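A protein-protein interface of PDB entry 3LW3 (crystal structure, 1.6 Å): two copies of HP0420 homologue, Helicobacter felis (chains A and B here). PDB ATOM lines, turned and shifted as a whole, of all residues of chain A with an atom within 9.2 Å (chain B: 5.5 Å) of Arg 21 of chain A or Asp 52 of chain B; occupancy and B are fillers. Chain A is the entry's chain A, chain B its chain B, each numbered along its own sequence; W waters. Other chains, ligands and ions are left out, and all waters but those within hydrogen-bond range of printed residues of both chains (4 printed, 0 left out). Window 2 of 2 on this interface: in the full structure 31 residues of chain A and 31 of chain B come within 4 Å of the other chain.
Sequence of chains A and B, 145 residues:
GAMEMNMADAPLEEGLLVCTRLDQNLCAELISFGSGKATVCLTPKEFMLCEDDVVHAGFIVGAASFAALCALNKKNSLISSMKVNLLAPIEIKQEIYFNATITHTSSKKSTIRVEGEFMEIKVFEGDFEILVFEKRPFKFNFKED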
ATOM      1  N   LEU A  16      -7.869  -3.059   9.495  1.00  0.00           N
ATOM      2  CA  LEU A  16      -7.671  -2.188   8.328  1.00  0.00           C
ATOM      3  C   LEU A  16      -7.882  -2.992   7.038  1.00  0.00           C
ATOM      4  O   LEU A  16      -7.134  -3.946   6.766  1.00  0.00           O
ATOM      5  CB  LEU A  16      -6.276  -1.598   8.342  1.00  0.00           C
ATOM      6  CG  LEU A  16      -6.154  -0.607   7.185  1.00  0.00           C
ATOM      7  CD1 LEU A  16      -6.942   0.652   7.549  1.00  0.00           C
ATOM      8  CD2 LEU A  16      -4.707  -0.290   6.915  1.00  0.00           C
ATOM      9  N   LEU A  17      -8.870  -2.617   6.227  1.00  0.00           N
ATOM     10  CA  LEU A  17      -9.277  -3.401   5.061  1.00  0.00           C
ATOM     11  C   LEU A  17      -8.726  -2.914   3.708  1.00  0.00           C
ATOM     12  O   LEU A  17      -9.015  -3.532   2.670  1.00  0.00           O
ATOM     13  CB  LEU A  17     -10.803  -3.453   4.958  1.00  0.00           C
ATOM     14  CG  LEU A  17     -11.604  -4.097   6.094  1.00  0.00           C
ATOM     15  CD1 LEU A  17     -13.088  -4.064   5.770  1.00  0.00           C
ATOM     16  CD2 LEU A  17     -11.169  -5.508   6.288  1.00  0.00           C
ATOM     17  N   VAL A  18      -7.970  -1.815   3.725  1.00  0.00           N
ATOM     18  CA  VAL A  18      -7.566  -1.143   2.484  1.00  0.00           C
ATOM     19  C   VAL A  18      -6.074  -1.026   2.334  1.00  0.00           C
ATOM     20  O   VAL A  18      -5.341  -0.975   3.331  1.00  0.00           O
ATOM     21  CB  VAL A  18      -8.129   0.307   2.384  1.00  0.00           C
ATOM     22  CG1 VAL A  18      -9.610   0.283   2.271  1.00  0.00           C
ATOM     23  CG2 VAL A  18      -7.605   1.158   3.545  1.00  0.00           C
ATOM     24  N   CYS A  19      -5.634  -0.974   1.072  1.00  0.00           N
ATOM     25  CA  CYS A  19      -4.218  -0.842   0.728  1.00  0.00           C
ATOM     26  C   CYS A  19      -3.299  -1.851   1.433  1.00  0.00           C
ATOM     27  O   CYS A  19      -2.281  -1.457   2.012  1.00  0.00           O
ATOM     28  CB  CYS A  19      -3.734   0.568   1.036  1.00  0.00           C
ATOM     29  SG  CYS A  19      -4.269   1.780  -0.159  1.00  0.00           S
ATOM     30  N   THR A  20      -3.622  -3.133   1.306  1.00  0.00           N
ATOM     31  CA  THR A  20      -2.826  -4.194   1.929  1.00  0.00           C
ATOM     32  C   THR A  20      -1.374  -4.194   1.442  1.00  0.00           C
ATOM     33  O   THR A  20      -0.477  -4.673   2.157  1.00  0.00           O
ATOM     34  CB  THR A  20      -3.452  -5.625   1.718  1.00  0.00           C
ATOM     35  OG1 THR A  20      -3.376  -6.021   0.338  1.00  0.00           O
ATOM     36  CG2 THR A  20      -4.904  -5.656   2.145  1.00  0.00           C
ATOM     37  N   ARG A  21      -1.123  -3.700   0.227  1.00  0.00           N
ATOM     38  CA  ARG A  21       0.223  -3.785  -0.349  1.00  0.00           C
ATOM     39  C   ARG A  21       1.023  -2.498  -0.196  1.00  0.00           C
ATOM     40  O   ARG A  21       2.157  -2.414  -0.655  1.00  0.00           O
ATOM     41  CB  ARG A  21       0.183  -4.195  -1.827  1.00  0.00           C
ATOM     42  CG  ARG A  21      -0.228  -5.666  -2.084  1.00  0.00           C
ATOM     43  CD  ARG A  21       0.979  -6.637  -2.056  1.00  0.00           C
ATOM     44  NE  ARG A  21       1.422  -7.116  -3.383  1.00  0.00           N
ATOM     45  CZ  ARG A  21       2.614  -6.847  -3.918  1.00  0.00           C
ATOM     46  NH1 ARG A  21       3.471  -6.048  -3.272  1.00  0.00           N
ATOM     47  NH2 ARG A  21       2.955  -7.357  -5.113  1.00  0.00           N
ATOM     48  N   LEU A  22       0.468  -1.502   0.480  1.00  0.00           N
ATOM     49  CA  LEU A  22       1.099  -0.179   0.468  1.00  0.00           C
ATOM     50  C   LEU A  22       2.302  -0.049   1.412  1.00  0.00           C
ATOM     51  O   LEU A  22       2.216  -0.417   2.572  1.00  0.00           O
ATOM     52  CB  LEU A  22       0.075   0.906   0.777  1.00  0.00           C
ATOM     53  CG  LEU A  22       0.534   2.355   0.623  1.00  0.00           C
ATOM     54  CD1 LEU A  22       0.010   2.983  -0.651  1.00  0.00           C
ATOM     55  CD2 LEU A  22      -0.025   3.084   1.790  1.00  0.00           C
ATOM     56  N   ASP A  23       3.409   0.486   0.922  1.00  0.00           N
ATOM     57  CA  ASP A  23       4.570   0.713   1.771  1.00  0.00           C
ATOM     58  C   ASP A  23       4.429   2.007   2.539  1.00  0.00           C
ATOM     59  O   ASP A  23       4.553   3.075   1.961  1.00  0.00           O
ATOM     60  CB  ASP A  23       5.833   0.780   0.930  1.00  0.00           C
ATOM     61  CG  ASP A  23       7.090   0.906   1.780  1.00  0.00           C
ATOM     62  OD1 ASP A  23       7.024   1.228   2.995  1.00  0.00           O
ATOM     63  OD2 ASP A  23       8.165   0.645   1.225  1.00  0.00           O
ATOM     64  N   GLN A  24       4.175   1.926   3.838  1.00  0.00           N
ATOM     65  CA  GLN A  24       3.946   3.154   4.589  1.00  0.00           C
ATOM     66  C   GLN A  24       5.176   4.041   4.635  1.00  0.00           C
ATOM     67  O   GLN A  24       5.019   5.263   4.755  1.00  0.00           O
ATOM     68  CB  GLN A  24       3.352   2.919   6.002  1.00  0.00           C
ATOM     69  CG  GLN A  24       1.881   2.495   5.967  1.00  0.00           C
ATOM     70  CD  GLN A  24       1.265   2.288   7.351  1.00  0.00           C
ATOM     71  OE1 GLN A  24       0.413   1.386   7.553  1.00  0.00           O
ATOM     72  NE2 GLN A  24       1.686   3.113   8.321  1.00  0.00           N
ATOM     73  N   ASN A  25       6.392   3.475   4.547  1.00  0.00           N
ATOM     74  CA  ASN A  25       7.566   4.369   4.551  1.00  0.00           C
ATOM     75  C   ASN A  25       7.598   5.266   3.328  1.00  0.00           C
ATOM     76  O   ASN A  25       8.137   6.383   3.378  1.00  0.00           O
ATOM     77  CB  ASN A  25       8.927   3.656   4.630  1.00  0.00           C
ATOM     78  CG  ASN A  25      10.120   4.663   4.469  1.00  0.00           C
ATOM     79  OD1 ASN A  25      10.250   5.626   5.242  1.00  0.00           O
ATOM     80  ND2 ASN A  25      10.963   4.451   3.450  1.00  0.00           N
ATOM     81  N   LEU A  26       7.045   4.776   2.223  1.00  0.00           N
ATOM     82  CA  LEU A  26       6.999   5.585   1.013  1.00  0.00           C
ATOM     83  C   LEU A  26       5.800   6.520   0.960  1.00  0.00           C
ATOM     84  O   LEU A  26       5.690   7.302   0.022  1.00  0.00           O
ATOM     85  CB  LEU A  26       7.003   4.692  -0.229  1.00  0.00           C
ATOM     86  CG  LEU A  26       8.253   3.818  -0.354  1.00  0.00           C
ATOM     87  CD1 LEU A  26       8.194   2.978  -1.632  1.00  0.00           C
ATOM     88  CD2 LEU A  26       9.550   4.645  -0.326  1.00  0.00           C
ATOM     89  N   CYS A  27       4.914   6.468   1.966  1.00  0.00           N
ATOM     90  CA  CYS A  27       3.637   7.195   1.909  1.00  0.00           C
ATOM     91  C   CYS A  27       3.434   7.991   3.189  1.00  0.00           C
ATOM     92  O   CYS A  27       3.714   9.152   3.225  1.00  0.00           O
ATOM     93  CB  CYS A  27       2.471   6.220   1.667  1.00  0.00           C
ATOM     94  SG  CYS A  27       0.837   6.971   1.530  1.00  0.00           S
ATOM     95  N   PHE A  66      -4.231   7.890   1.020  1.00  0.00           N
ATOM     96  CA  PHE A  66      -4.180   6.826   2.013  1.00  0.00           C
ATOM     97  C   PHE A  66      -5.110   7.165   3.184  1.00  0.00           C
ATOM     98  O   PHE A  66      -5.922   6.329   3.581  1.00  0.00           O
ATOM     99  CB  PHE A  66      -2.737   6.621   2.452  1.00  0.00           C
ATOM    100  CG  PHE A  66      -2.551   5.525   3.471  1.00  0.00           C
ATOM    101  CD1 PHE A  66      -3.209   4.310   3.349  1.00  0.00           C
ATOM    102  CD2 PHE A  66      -1.653   5.708   4.534  1.00  0.00           C
ATOM    103  CE1 PHE A  66      -2.974   3.271   4.315  1.00  0.00           C
ATOM    104  CE2 PHE A  66      -1.445   4.738   5.458  1.00  0.00           C
ATOM    105  CZ  PHE A  66      -2.115   3.521   5.358  1.00  0.00           C
ATOM    106  N   LYS A  75     -13.185  -2.931   1.794  1.00  0.00           N
ATOM    107  CA  LYS A  75     -12.540  -3.817   0.856  1.00  0.00           C
ATOM    108  C   LYS A  75     -13.063  -3.484  -0.530  1.00  0.00           C
ATOM    109  O   LYS A  75     -14.197  -3.009  -0.676  1.00  0.00           O
ATOM    110  CB  LYS A  75     -12.923  -5.250   1.215  1.00  0.00           C
ATOM    111  CG  LYS A  75     -12.374  -6.315   0.286  1.00  0.00           C
ATOM    112  CD  LYS A  75     -11.075  -6.962   0.857  1.00  0.00           C
ATOM    113  CE  LYS A  75     -10.654  -8.273   0.094  1.00  0.00           C
ATOM    114  NZ  LYS A  75      -9.910  -8.038  -1.229  1.00  0.00           N
ATOM    115  N   GLU B  46       6.226  -2.628  -8.112  1.00  0.00           N
ATOM    116  CA  GLU B  46       5.598  -3.205  -6.931  1.00  0.00           C
ATOM    117  C   GLU B  46       5.486  -2.243  -5.756  1.00  0.00           C
ATOM    118  O   GLU B  46       4.434  -2.221  -5.088  1.00  0.00           O
ATOM    119  CB  GLU B  46       6.303  -4.488  -6.513  1.00  0.00           C
ATOM    120  CG  GLU B  46       5.854  -5.636  -7.363  1.00  0.00           C
ATOM    121  CD  GLU B  46       6.764  -6.870  -7.247  1.00  0.00           C
ATOM    122  OE1 GLU B  46       7.252  -7.142  -6.113  1.00  0.00           O
ATOM    123  OE2 GLU B  46       6.990  -7.549  -8.292  1.00  0.00           O
ATOM    124  N   LEU B  49       2.164  -0.060  -5.389  1.00  0.00           N
ATOM    125  CA  LEU B  49       0.833  -0.667  -5.215  1.00  0.00           C
ATOM    126  C   LEU B  49       0.130  -0.236  -3.937  1.00  0.00           C
ATOM    127  O   LEU B  49       0.757  -0.127  -2.866  1.00  0.00           O
ATOM    128  CB  LEU B  49       0.967  -2.192  -5.194  1.00  0.00           C
ATOM    129  CG  LEU B  49       1.347  -2.795  -6.543  1.00  0.00           C
ATOM    130  CD1 LEU B  49       1.704  -4.267  -6.363  1.00  0.00           C
ATOM    131  CD2 LEU B  49       0.275  -2.610  -7.608  1.00  0.00           C
ATOM    132  N   CYS B  50      -1.178   0.003  -4.044  1.00  0.00           N
ATOM    133  CA  CYS B  50      -2.041   0.111  -2.872  1.00  0.00           C
ATOM    134  C   CYS B  50      -2.551  -1.280  -2.564  1.00  0.00           C
ATOM    135  O   CYS B  50      -2.359  -1.780  -1.460  1.00  0.00           O
ATOM    136  CB  CYS B  50      -3.206   1.040  -3.163  1.00  0.00           C
ATOM    137  SG  CYS B  50      -4.592   0.960  -1.997  1.00  0.00           S
ATOM    138  N   GLU B  51      -3.196  -1.889  -3.541  1.00  0.00           N
ATOM    139  CA  GLU B  51      -3.660  -3.288  -3.443  1.00  0.00           C
ATOM    140  C   GLU B  51      -2.857  -4.152  -4.417  1.00  0.00           C
ATOM    141  O   GLU B  51      -2.101  -3.631  -5.238  1.00  0.00           O
ATOM    142  CB  GLU B  51      -5.176  -3.439  -3.756  1.00  0.00           C
ATOM    143  CG  GLU B  51      -6.117  -2.351  -3.173  1.00  0.00           C
ATOM    144  CD  GLU B  51      -6.513  -2.621  -1.722  1.00  0.00           C
ATOM    145  OE1 GLU B  51      -5.996  -3.614  -1.164  1.00  0.00           O
ATOM    146  OE2 GLU B  51      -7.280  -1.816  -1.138  1.00  0.00           O
ATOM    147  N   ASP B  52      -3.010  -5.479  -4.319  1.00  0.00           N
ATOM    148  CA  ASP B  52      -2.376  -6.378  -5.280  1.00  0.00           C
ATOM    149  C   ASP B  52      -2.521  -5.895  -6.743  1.00  0.00           C
ATOM    150  O   ASP B  52      -1.574  -6.002  -7.526  1.00  0.00           O
ATOM    151  CB  ASP B  52      -3.032  -7.759  -5.185  1.00  0.00           C
ATOM    152  CG  ASP B  52      -2.521  -8.573  -4.021  1.00  0.00           C
ATOM    153  OD1 ASP B  52      -3.239  -9.515  -3.620  1.00  0.00           O
ATOM    154  OD2 ASP B  52      -1.396  -8.325  -3.534  1.00  0.00           O
ATOM    155  N   ASP B  53      -3.716  -5.427  -7.108  1.00  0.00           N
ATOM    156  CA  ASP B  53      -4.067  -5.090  -8.499  1.00  0.00           C
ATOM    157  C   ASP B  53      -4.446  -3.613  -8.688  1.00  0.00           C
ATOM    158  O   ASP B  53      -5.125  -3.237  -9.673  1.00  0.00           O
ATOM    159  CB  ASP B  53      -5.248  -5.954  -8.957  1.00  0.00           C
ATOM    160  CG  ASP B  53      -6.338  -6.100  -7.872  1.00  0.00           C
ATOM    161  OD1 ASP B  53      -6.204  -5.568  -6.718  1.00  0.00           O
ATOM    162  OD2 ASP B  53      -7.356  -6.791  -8.179  1.00  0.00           O
ATOM    163  N   VAL B  54      -4.005  -2.772  -7.752  1.00  0.00           N
ATOM    164  CA  VAL B  54      -4.307  -1.361  -7.824  1.00  0.00           C
ATOM    165  C   VAL B  54      -3.131  -0.481  -7.418  1.00  0.00           C
ATOM    166  O   VAL B  54      -2.704  -0.437  -6.230  1.00  0.00           O
ATOM    167  CB  VAL B  54      -5.536  -0.970  -6.958  1.00  0.00           C
ATOM    168  CG1 VAL B  54      -5.873   0.485  -7.198  1.00  0.00           C
ATOM    169  CG2 VAL B  54      -6.760  -1.901  -7.246  1.00  0.00           C
HETATM  170  O   HOH W   1      -8.077  -4.397   0.555  1.00  0.00           O
HETATM  171  O   HOH W   2       3.105   1.356  -1.913  1.00  0.00           O
HETATM  172  O   HOH W   3       4.215  -2.815  -2.314  1.00  0.00           O
HETATM  173  O   HOH W   4      -4.823  -6.100  -2.047  1.00  0.00           O
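N of Thr 20 of chain A lies within hydrogen-bond range of OE1 of Glu 51 of chain B (3.5 Å).
The backbone carbonyl oxygen of Leu 49 of chain B lies close to the backbone carbonyl oxygen of Arg 21 of chain A (3.5 Å).
The guanidinium group (NE) of Arg 21 of chain A is in salt-bridge range of the side-chain carboxylate (OD2) of Asp 52 of chain B (3.1 Å).
O of Cys 50 of chain B lies within hydrogen-bond range of N of Leu 22 of chain A, at 3.4 Å.
The backbone NH of Cys 19 of chain A lies within hydrogen-bond range of the side-chain carboxylate of Glu 51 of chain B, 2.9 Å away.
O of Cys 50 of chain B is in hydrogen-bond range of N of Thr 20 of chain A (3.3 Å).
The backbone NH (N) of Arg 21 of chain A lies within hydrogen-bond range of the backbone carbonyl oxygen (O) of Cys 50 of chain B (2.8 Å).
The side-chain sulfur of Cys 19 of chain A forms a disulfide with the side-chain sulfur of Cys 50 of chain B, 2.0 Å away.
Among the printed residues, pairs that only touch across the chains: Leu 22 of chain A with Leu 49 of chain B (3.4 Å), Val 18 of chain A with Glu 51 of chain B (3.7 Å) and Arg 21 of chain A with Glu 51 of chain B (3.8 Å).
Of the printed residues of chain B, Cys 19 of chain A touches Cys 50 (2.0 Å) and Glu 51 (2.9 Å).
Arg 21 of chain A touches just these residues of chain B: Leu 49 (3.5 Å), Cys 50 (2.8 Å), Glu 51 (3.8 Å) and Asp 52 (3.1 Å).
Of the printed residues of chain B, Leu 22 of chain A touches Leu 49 and Cys 50.
Leu 26 of chain A touches none of the printed residues of chain B.
Of the printed residues of chain A, Leu 49 of chain B touches Arg 21 and Leu 22.
Of chain A, only Arg 21 (3.1 Å) comes within 4 Å of Asp 52 of chain B.
The nearest residue of chain B that does not touch Arg 21 of chain A is Glu 46 of chain B (4.1 Å).
The nearest printed residue of chain B that does not touch Leu 22 of chain A is Glu 51 of chain B (5.5 Å).
Printed residues of chain A that touch a printed residue of chain B: Val 18, Cys 19, Thr 20, Arg 21 and Leu 22.
Hydrophobic or aromatic side chains of chain A that line the printed part of chain B: Leu 22.
Hydrophobic or aromatic side chains of chain B within 4 Å of the printed part of chain A: Leu 49.
Among the printed residues, 11 pairs touch across the chains.
No position is printed for both chains.
Of the 11 pairs that touch across the chains among the printed residues, none has its exchanged pair printed and touching as well.
Water W1 lies within hydrogen-bond range of the backbone carbonyl oxygen of Leu 17 of chain A (2.5 Å) and the side-chain carboxylate of Glu 51 of chain B (2.8 Å).
Water W3 bridges the backbone carbonyl oxygen (O) of Arg 21 of chain A and the backbone carbonyl oxygen (O) of Glu 46 of chain B.
Water W4 lies within hydrogen-bond range of OG1 of Thr 20 of chain A (2.8 Å), OE1 of Glu 51 of chain B (2.9 Å) and N of Asp 52 of chain B (3.0 Å).
Water W2 bridges the backbone carbonyl oxygen of Leu 49 of chain B (2.9 Å) and the backbone NH of Asp 23 of chain A (3.0 Å).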
